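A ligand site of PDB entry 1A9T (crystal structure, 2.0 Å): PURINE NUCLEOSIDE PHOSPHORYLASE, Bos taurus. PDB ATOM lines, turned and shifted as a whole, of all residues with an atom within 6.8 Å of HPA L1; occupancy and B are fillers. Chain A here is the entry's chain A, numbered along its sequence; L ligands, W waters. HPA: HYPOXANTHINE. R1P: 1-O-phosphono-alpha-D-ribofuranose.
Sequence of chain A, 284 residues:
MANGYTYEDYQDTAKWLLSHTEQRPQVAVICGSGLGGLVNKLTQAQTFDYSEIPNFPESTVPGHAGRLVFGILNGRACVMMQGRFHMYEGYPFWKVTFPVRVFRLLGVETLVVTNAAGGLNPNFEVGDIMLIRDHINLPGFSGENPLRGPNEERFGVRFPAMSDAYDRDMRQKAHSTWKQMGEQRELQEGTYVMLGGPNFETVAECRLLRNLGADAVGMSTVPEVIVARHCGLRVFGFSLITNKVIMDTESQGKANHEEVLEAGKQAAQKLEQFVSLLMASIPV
N1 of HPA L1 is in hydrogen-bond range of OE1 of Glu 201, 2.8 Å away.
The backbone carbonyl oxygen (O) of Ala 116 lies close to a nitrogen (N9) of HPA L1 (3.3 Å).
N of Gly 118 lies close to N7 of HPA L1.
N of Met 219 is in hydrogen-bond range of O2 of R1P L2.
The side-chain amide oxygen (OD1) of Asn 243 lies within hydrogen-bond range of a nitrogen (N7) of HPA L1 (2.8 Å).
The backbone NH (N) of Ala 116 sits at hydrogen-bond distance from an oxygen (O2P) of R1P L2, at 2.9 Å.
N of Ala 117 is in hydrogen-bond range of O of Leu 240, at 2.9 Å.
The backbone NH (N) of Gly 118 sits at hydrogen-bond distance from the backbone carbonyl oxygen (O) of Val 217, 2.9 Å away.
The backbone carbonyl oxygen (O) of Gly 218 sits at hydrogen-bond distance from the backbone NH (N) of Leu 195, at 3.1 Å.
The side-chain amide oxygen (OD1) of Asn 243 sits at hydrogen-bond distance from the side-chain hydroxyl (OG1) of Thr 242.
N of Thr 242 is in hydrogen-bond range of O of Ala 117 (3.1 Å).
N of Gly 119 sits at hydrogen-bond distance from O of Asn 243 (2.8 Å).
N of Met 219 sits at hydrogen-bond distance from OH of Tyr 192 (3.4 Å).
Ala 117 touches HPA L1 (C to C8, 3.6 Å).
Phe 200 touches HPA L1.
O of Val 217 touches N3 of HPA L1, at 3.5 Å.
Gly 218 touches HPA L1.
Met 219 touches HPA L1.
OG1 of Thr 242 touches C8 of HPA L1, at 3.5 Å.
Ten residues have an atom within 4 Å of HPA L1: Ala 116, Ala 117, Gly 118, Phe 200, Glu 201, Val 217, Gly 218, Met 219, Thr 242 and Asn 243.
Along chain A the residues within 4 Å of HPA L1 span positions 116 to 243.
The nearest printed residue that does not touch HPA L1 is Val 245 (4.2 Å).
Water W1 lies within hydrogen-bond range of the side-chain carboxylate (OE1) of Glu 201 (2.7 Å) and an oxygen (O6) of HPA L1 (3.0 Å).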
ATOM      1  N   ASN A 115       1.404 -10.274 -20.823  1.00  0.00           N
ATOM      2  CA  ASN A 115       1.851  -9.129 -20.041  1.00  0.00           C
ATOM      3  C   ASN A 115       0.654  -8.297 -19.624  1.00  0.00           C
ATOM      4  O   ASN A 115      -0.467  -8.541 -20.068  1.00  0.00           O
ATOM      5  CB  ASN A 115       2.846  -8.272 -20.838  1.00  0.00           C
ATOM      6  CG  ASN A 115       2.239  -7.683 -22.107  1.00  0.00           C
ATOM      7  OD1 ASN A 115       1.240  -6.971 -22.063  1.00  0.00           O
ATOM      8  ND2 ASN A 115       2.861  -7.967 -23.251  1.00  0.00           N
ATOM      9  N   ALA A 116       0.898  -7.377 -18.706  1.00  0.00           N
ATOM     10  CA  ALA A 116      -0.102  -6.462 -18.214  1.00  0.00           C
ATOM     11  C   ALA A 116       0.310  -5.184 -18.945  1.00  0.00           C
ATOM     12  O   ALA A 116       1.500  -4.882 -18.992  1.00  0.00           O
ATOM     13  CB  ALA A 116       0.038  -6.282 -16.704  1.00  0.00           C
ATOM     14  N   ALA A 117      -0.641  -4.481 -19.555  1.00  0.00           N
ATOM     15  CA  ALA A 117      -0.297  -3.271 -20.286  1.00  0.00           C
ATOM     16  C   ALA A 117      -1.288  -2.152 -20.022  1.00  0.00           C
ATOM     17  O   ALA A 117      -2.430  -2.390 -19.643  1.00  0.00           O
ATOM     18  CB  ALA A 117      -0.226  -3.544 -21.786  1.00  0.00           C
ATOM     19  N   GLY A 118      -0.823  -0.920 -20.226  1.00  0.00           N
ATOM     20  CA  GLY A 118      -1.673   0.237 -20.045  1.00  0.00           C
ATOM     21  C   GLY A 118      -2.392   0.436 -21.362  1.00  0.00           C
ATOM     22  O   GLY A 118      -1.799   0.263 -22.430  1.00  0.00           O
ATOM     23  N   GLY A 119      -3.669   0.785 -21.287  1.00  0.00           N
ATOM     24  CA  GLY A 119      -4.445   0.977 -22.490  1.00  0.00           C
ATOM     25  C   GLY A 119      -4.314   2.360 -23.106  1.00  0.00           C
ATOM     26  O   GLY A 119      -4.463   3.367 -22.409  1.00  0.00           O
ATOM     27  N   TYR A 192       1.398  -3.393 -29.633  1.00  0.00           N
ATOM     28  CA  TYR A 192       1.964  -3.196 -28.320  1.00  0.00           C
ATOM     29  C   TYR A 192       3.242  -2.365 -28.472  1.00  0.00           C
ATOM     30  O   TYR A 192       4.050  -2.630 -29.367  1.00  0.00           O
ATOM     31  CB  TYR A 192       2.281  -4.564 -27.699  1.00  0.00           C
ATOM     32  CG  TYR A 192       3.000  -4.536 -26.386  1.00  0.00           C
ATOM     33  CD1 TYR A 192       4.397  -4.539 -26.327  1.00  0.00           C
ATOM     34  CD2 TYR A 192       2.297  -4.536 -25.186  1.00  0.00           C
ATOM     35  CE1 TYR A 192       5.069  -4.550 -25.124  1.00  0.00           C
ATOM     36  CE2 TYR A 192       2.966  -4.557 -23.960  1.00  0.00           C
ATOM     37  CZ  TYR A 192       4.346  -4.566 -23.938  1.00  0.00           C
ATOM     38  OH  TYR A 192       5.002  -4.612 -22.749  1.00  0.00           O
ATOM     39  N   LEU A 195       8.561   0.410 -23.880  1.00  0.00           N
ATOM     40  CA  LEU A 195       9.458   1.474 -23.473  1.00  0.00           C
ATOM     41  C   LEU A 195      10.201   0.957 -22.228  1.00  0.00           C
ATOM     42  O   LEU A 195       9.799  -0.050 -21.652  1.00  0.00           O
ATOM     43  CB  LEU A 195       8.722   2.808 -23.210  1.00  0.00           C
ATOM     44  CG  LEU A 195       7.345   2.902 -22.555  1.00  0.00           C
ATOM     45  CD1 LEU A 195       7.355   2.324 -21.132  1.00  0.00           C
ATOM     46  CD2 LEU A 195       6.929   4.389 -22.545  1.00  0.00           C
ATOM     47  N   ASN A 199       9.337   4.085 -14.434  1.00  0.00           N
ATOM     48  CA  ASN A 199       8.308   5.084 -14.130  1.00  0.00           C
ATOM     49  C   ASN A 199       7.155   4.974 -15.114  1.00  0.00           C
ATOM     50  O   ASN A 199       7.310   4.437 -16.212  1.00  0.00           O
ATOM     51  CB  ASN A 199       8.876   6.515 -14.180  1.00  0.00           C
ATOM     52  CG  ASN A 199       9.383   6.889 -15.558  1.00  0.00           C
ATOM     53  OD1 ASN A 199      10.526   6.583 -15.919  1.00  0.00           O
ATOM     54  ND2 ASN A 199       8.549   7.557 -16.341  1.00  0.00           N
ATOM     55  N   PHE A 200       6.002   5.495 -14.723  1.00  0.00           N
ATOM     56  CA  PHE A 200       4.843   5.484 -15.584  1.00  0.00           C
ATOM     57  C   PHE A 200       4.893   6.760 -16.440  1.00  0.00           C
ATOM     58  O   PHE A 200       5.573   7.718 -16.081  1.00  0.00           O
ATOM     59  CB  PHE A 200       3.546   5.358 -14.788  1.00  0.00           C
ATOM     60  CG  PHE A 200       3.305   3.964 -14.252  1.00  0.00           C
ATOM     61  CD1 PHE A 200       3.170   2.888 -15.122  1.00  0.00           C
ATOM     62  CD2 PHE A 200       3.182   3.732 -12.891  1.00  0.00           C
ATOM     63  CE1 PHE A 200       2.932   1.605 -14.650  1.00  0.00           C
ATOM     64  CE2 PHE A 200       2.934   2.457 -12.408  1.00  0.00           C
ATOM     65  CZ  PHE A 200       2.808   1.383 -13.280  1.00  0.00           C
ATOM     66  N   GLU A 201       4.171   6.755 -17.550  1.00  0.00           N
ATOM     67  CA  GLU A 201       4.178   7.839 -18.519  1.00  0.00           C
ATOM     68  C   GLU A 201       3.517   9.177 -18.149  1.00  0.00           C
ATOM     69  O   GLU A 201       2.666   9.257 -17.256  1.00  0.00           O
ATOM     70  CB  GLU A 201       3.595   7.328 -19.847  1.00  0.00           C
ATOM     71  CG  GLU A 201       4.278   6.082 -20.457  1.00  0.00           C
ATOM     72  CD  GLU A 201       3.995   4.776 -19.686  1.00  0.00           C
ATOM     73  OE1 GLU A 201       2.845   4.591 -19.240  1.00  0.00           O
ATOM     74  OE2 GLU A 201       4.907   3.942 -19.536  1.00  0.00           O
ATOM     75  N   CYS A 206       1.970   9.772 -23.446  1.00  0.00           N
ATOM     76  CA  CYS A 206       0.847   8.914 -23.812  1.00  0.00           C
ATOM     77  C   CYS A 206       0.165   9.350 -25.101  1.00  0.00           C
ATOM     78  O   CYS A 206      -0.166   8.518 -25.940  1.00  0.00           O
ATOM     79  CB  CYS A 206      -0.158   8.860 -22.660  1.00  0.00           C
ATOM     80  SG  CYS A 206       0.383   7.841 -21.270  1.00  0.00           S
ATOM     81  N   VAL A 217       0.655   0.020 -23.973  1.00  0.00           N
ATOM     82  CA  VAL A 217       2.048   0.291 -23.646  1.00  0.00           C
ATOM     83  C   VAL A 217       2.510  -0.608 -22.500  1.00  0.00           C
ATOM     84  O   VAL A 217       1.717  -0.905 -21.588  1.00  0.00           O
ATOM     85  CB  VAL A 217       2.248   1.793 -23.295  1.00  0.00           C
ATOM     86  CG1 VAL A 217       1.350   2.209 -22.123  1.00  0.00           C
ATOM     87  CG2 VAL A 217       3.710   2.069 -22.983  1.00  0.00           C
ATOM     88  N   GLY A 218       3.772  -1.041 -22.543  1.00  0.00           N
ATOM     89  CA  GLY A 218       4.305  -1.899 -21.507  1.00  0.00           C
ATOM     90  C   GLY A 218       5.828  -1.831 -21.470  1.00  0.00           C
ATOM     91  O   GLY A 218       6.428  -1.175 -22.323  1.00  0.00           O
ATOM     92  N   MET A 219       6.435  -2.544 -20.526  1.00  0.00           N
ATOM     93  CA  MET A 219       7.894  -2.524 -20.349  1.00  0.00           C
ATOM     94  C   MET A 219       8.580  -3.886 -20.527  1.00  0.00           C
ATOM     95  O   MET A 219       9.588  -4.180 -19.860  1.00  0.00           O
ATOM     96  CB  MET A 219       8.224  -1.986 -18.945  1.00  0.00           C
ATOM     97  CG  MET A 219       7.536  -0.675 -18.586  1.00  0.00           C
ATOM     98  SD  MET A 219       7.624  -0.285 -16.813  1.00  0.00           S
ATOM     99  CE  MET A 219       6.664   1.221 -16.730  1.00  0.00           C
ATOM    100  N   LEU A 240      -3.096  -7.961 -21.007  1.00  0.00           N
ATOM    101  CA  LEU A 240      -4.281  -7.810 -20.180  1.00  0.00           C
ATOM    102  C   LEU A 240      -4.254  -6.305 -19.940  1.00  0.00           C
ATOM    103  O   LEU A 240      -3.241  -5.775 -19.456  1.00  0.00           O
ATOM    104  CB  LEU A 240      -4.117  -8.552 -18.841  1.00  0.00           C
ATOM    105  CG  LEU A 240      -5.166  -8.180 -17.788  1.00  0.00           C
ATOM    106  CD1 LEU A 240      -6.529  -8.676 -18.208  1.00  0.00           C
ATOM    107  CD2 LEU A 240      -4.785  -8.756 -16.436  1.00  0.00           C
ATOM    108  N   THR A 242      -4.726  -3.569 -17.884  1.00  0.00           N
ATOM    109  CA  THR A 242      -4.924  -3.351 -16.446  1.00  0.00           C
ATOM    110  C   THR A 242      -5.388  -1.963 -16.036  1.00  0.00           C
ATOM    111  O   THR A 242      -5.916  -1.773 -14.941  1.00  0.00           O
ATOM    112  CB  THR A 242      -3.649  -3.676 -15.642  1.00  0.00           C
ATOM    113  OG1 THR A 242      -2.536  -2.916 -16.144  1.00  0.00           O
ATOM    114  CG2 THR A 242      -3.335  -5.162 -15.735  1.00  0.00           C
ATOM    115  N   ASN A 243      -5.200  -0.995 -16.916  1.00  0.00           N
ATOM    116  CA  ASN A 243      -5.594   0.374 -16.589  1.00  0.00           C
ATOM    117  C   ASN A 243      -5.647   1.209 -17.848  1.00  0.00           C
ATOM    118  O   ASN A 243      -5.041   0.888 -18.862  1.00  0.00           O
ATOM    119  CB  ASN A 243      -4.579   0.986 -15.623  1.00  0.00           C
ATOM    120  CG  ASN A 243      -3.168   1.039 -16.208  1.00  0.00           C
ATOM    121  OD1 ASN A 243      -2.536   0.003 -16.401  1.00  0.00           O
ATOM    122  ND2 ASN A 243      -2.684   2.238 -16.504  1.00  0.00           N
ATOM    123  N   LYS A 244      -6.408   2.300 -17.759  1.00  0.00           N
ATOM    124  CA  LYS A 244      -6.523   3.233 -18.863  1.00  0.00           C
ATOM    125  C   LYS A 244      -5.517   4.334 -18.593  1.00  0.00           C
ATOM    126  O   LYS A 244      -5.443   4.885 -17.489  1.00  0.00           O
ATOM    127  CB  LYS A 244      -7.938   3.806 -18.950  1.00  0.00           C
ATOM    128  CG  LYS A 244      -8.996   2.822 -19.437  1.00  0.00           C
ATOM    129  CD  LYS A 244      -8.680   2.335 -20.848  1.00  0.00           C
ATOM    130  CE  LYS A 244      -8.686   3.486 -21.853  1.00  0.00           C
ATOM    131  NZ  LYS A 244      -8.159   3.075 -23.180  1.00  0.00           N
ATOM    132  N   VAL A 245      -4.682   4.595 -19.592  1.00  0.00           N
ATOM    133  CA  VAL A 245      -3.649   5.619 -19.513  1.00  0.00           C
ATOM    134  C   VAL A 245      -4.259   7.028 -19.365  1.00  0.00           C
ATOM    135  O   VAL A 245      -5.264   7.356 -19.985  1.00  0.00           O
ATOM    136  CB  VAL A 245      -2.755   5.517 -20.760  1.00  0.00           C
ATOM    137  CG1 VAL A 245      -2.274   6.871 -21.195  1.00  0.00           C
ATOM    138  CG2 VAL A 245      -1.596   4.585 -20.493  1.00  0.00           C
ATOM    139  N   ALA A 255      -1.485   5.957 -12.531  1.00  0.00           N
ATOM    140  CA  ALA A 255      -1.083   4.557 -12.569  1.00  0.00           C
ATOM    141  C   ALA A 255      -0.237   4.145 -11.366  1.00  0.00           C
ATOM    142  O   ALA A 255       0.597   4.910 -10.883  1.00  0.00           O
ATOM    143  CB  ALA A 255      -0.343   4.251 -13.866  1.00  0.00           C
ATOM    144  N   ASN A 256      -0.466   2.914 -10.901  1.00  0.00           N
ATOM    145  CA  ASN A 256       0.242   2.352  -9.767  1.00  0.00           C
ATOM    146  C   ASN A 256       0.324   0.836  -9.946  1.00  0.00           C
ATOM    147  O   ASN A 256      -0.585   0.232 -10.513  1.00  0.00           O
ATOM    148  CB  ASN A 256      -0.462   2.699  -8.451  1.00  0.00           C
ATOM    149  CG  ASN A 256      -1.843   2.087  -8.353  1.00  0.00           C
ATOM    150  OD1 ASN A 256      -2.016   1.023  -7.743  1.00  0.00           O
ATOM    151  ND2 ASN A 256      -2.830   2.741  -8.941  1.00  0.00           N
ATOM    152  N   GLU A 259      -2.587  -1.628  -8.583  1.00  0.00           N
ATOM    153  CA  GLU A 259      -3.808  -1.630  -9.382  1.00  0.00           C
ATOM    154  C   GLU A 259      -3.671  -2.637 -10.517  1.00  0.00           C
ATOM    155  O   GLU A 259      -4.640  -3.323 -10.870  1.00  0.00           O
ATOM    156  CB  GLU A 259      -4.107  -0.221  -9.928  1.00  0.00           C
ATOM    157  CG  GLU A 259      -3.802  -0.048 -11.430  1.00  0.00           C
ATOM    158  CD  GLU A 259      -3.832   1.399 -11.899  1.00  0.00           C
ATOM    159  OE1 GLU A 259      -4.865   2.092 -11.694  1.00  0.00           O
ATOM    160  OE2 GLU A 259      -2.825   1.849 -12.491  1.00  0.00           O
ATOM    161  N   VAL A 260      -2.486  -2.741 -11.103  1.00  0.00           N
ATOM    162  CA  VAL A 260      -2.277  -3.697 -12.196  1.00  0.00           C
ATOM    163  C   VAL A 260      -2.331  -5.129 -11.661  1.00  0.00           C
ATOM    164  O   VAL A 260      -2.927  -6.011 -12.280  1.00  0.00           O
ATOM    165  CB  VAL A 260      -0.968  -3.446 -12.999  1.00  0.00           C
ATOM    166  CG1 VAL A 260      -0.676  -1.950 -13.095  1.00  0.00           C
ATOM    167  CG2 VAL A 260       0.189  -4.237 -12.449  1.00  0.00           C
HETATM  168  N1  HPA L   1       2.380   1.935 -18.440  1.00  0.00           N
HETATM  169  C2  HPA L   1       3.417   1.119 -18.807  1.00  0.00           C
HETATM  170  N3  HPA L   1       3.385  -0.204 -18.585  1.00  0.00           N
HETATM  171  C4  HPA L   1       2.208  -0.621 -17.975  1.00  0.00           C
HETATM  172  C5  HPA L   1       1.144   0.148 -17.587  1.00  0.00           C
HETATM  173  C6  HPA L   1       1.169   1.541 -17.816  1.00  0.00           C
HETATM  174  O6  HPA L   1       0.273   2.354 -17.527  1.00  0.00           O
HETATM  175  N7  HPA L   1       0.176  -0.624 -17.009  1.00  0.00           N
HETATM  176  C8  HPA L   1       0.665  -1.900 -17.046  1.00  0.00           C
HETATM  177  N9  HPA L   1       1.897  -1.941 -17.638  1.00  0.00           N
HETATM  178  C5  R1P L   2       3.470  -2.084 -14.259  1.00  0.00           C
HETATM  179  O5  R1P L   2       2.400  -2.295 -13.231  1.00  0.00           O
HETATM  180  C4  R1P L   2       4.387  -3.169 -14.686  1.00  0.00           C
HETATM  181  O4  R1P L   2       3.476  -4.218 -15.287  1.00  0.00           O
HETATM  182  C1  R1P L   2       3.843  -4.716 -16.574  1.00  0.00           C
HETATM  183  C2  R1P L   2       4.874  -3.540 -17.023  1.00  0.00           C
HETATM  184  O2  R1P L   2       5.825  -4.003 -17.996  1.00  0.00           O
HETATM  185  C3  R1P L   2       5.531  -2.972 -15.727  1.00  0.00           C
HETATM  186  O3  R1P L   2       6.695  -3.757 -15.425  1.00  0.00           O
HETATM  187  O1  R1P L   2       4.909  -5.990 -16.312  1.00  0.00           O
HETATM  188  P   R1P L   2       4.966  -7.295 -17.451  1.00  0.00           P
HETATM  189  O1P R1P L   2       5.961  -8.383 -17.084  1.00  0.00           O
HETATM  190  O2P R1P L   2       3.495  -7.598 -17.350  1.00  0.00           O
HETATM  191  O3P R1P L   2       5.152  -6.613 -18.780  1.00  0.00           O
HETATM  192  O   HOH W   1       0.870   5.274 -17.592  1.00  0.00           O
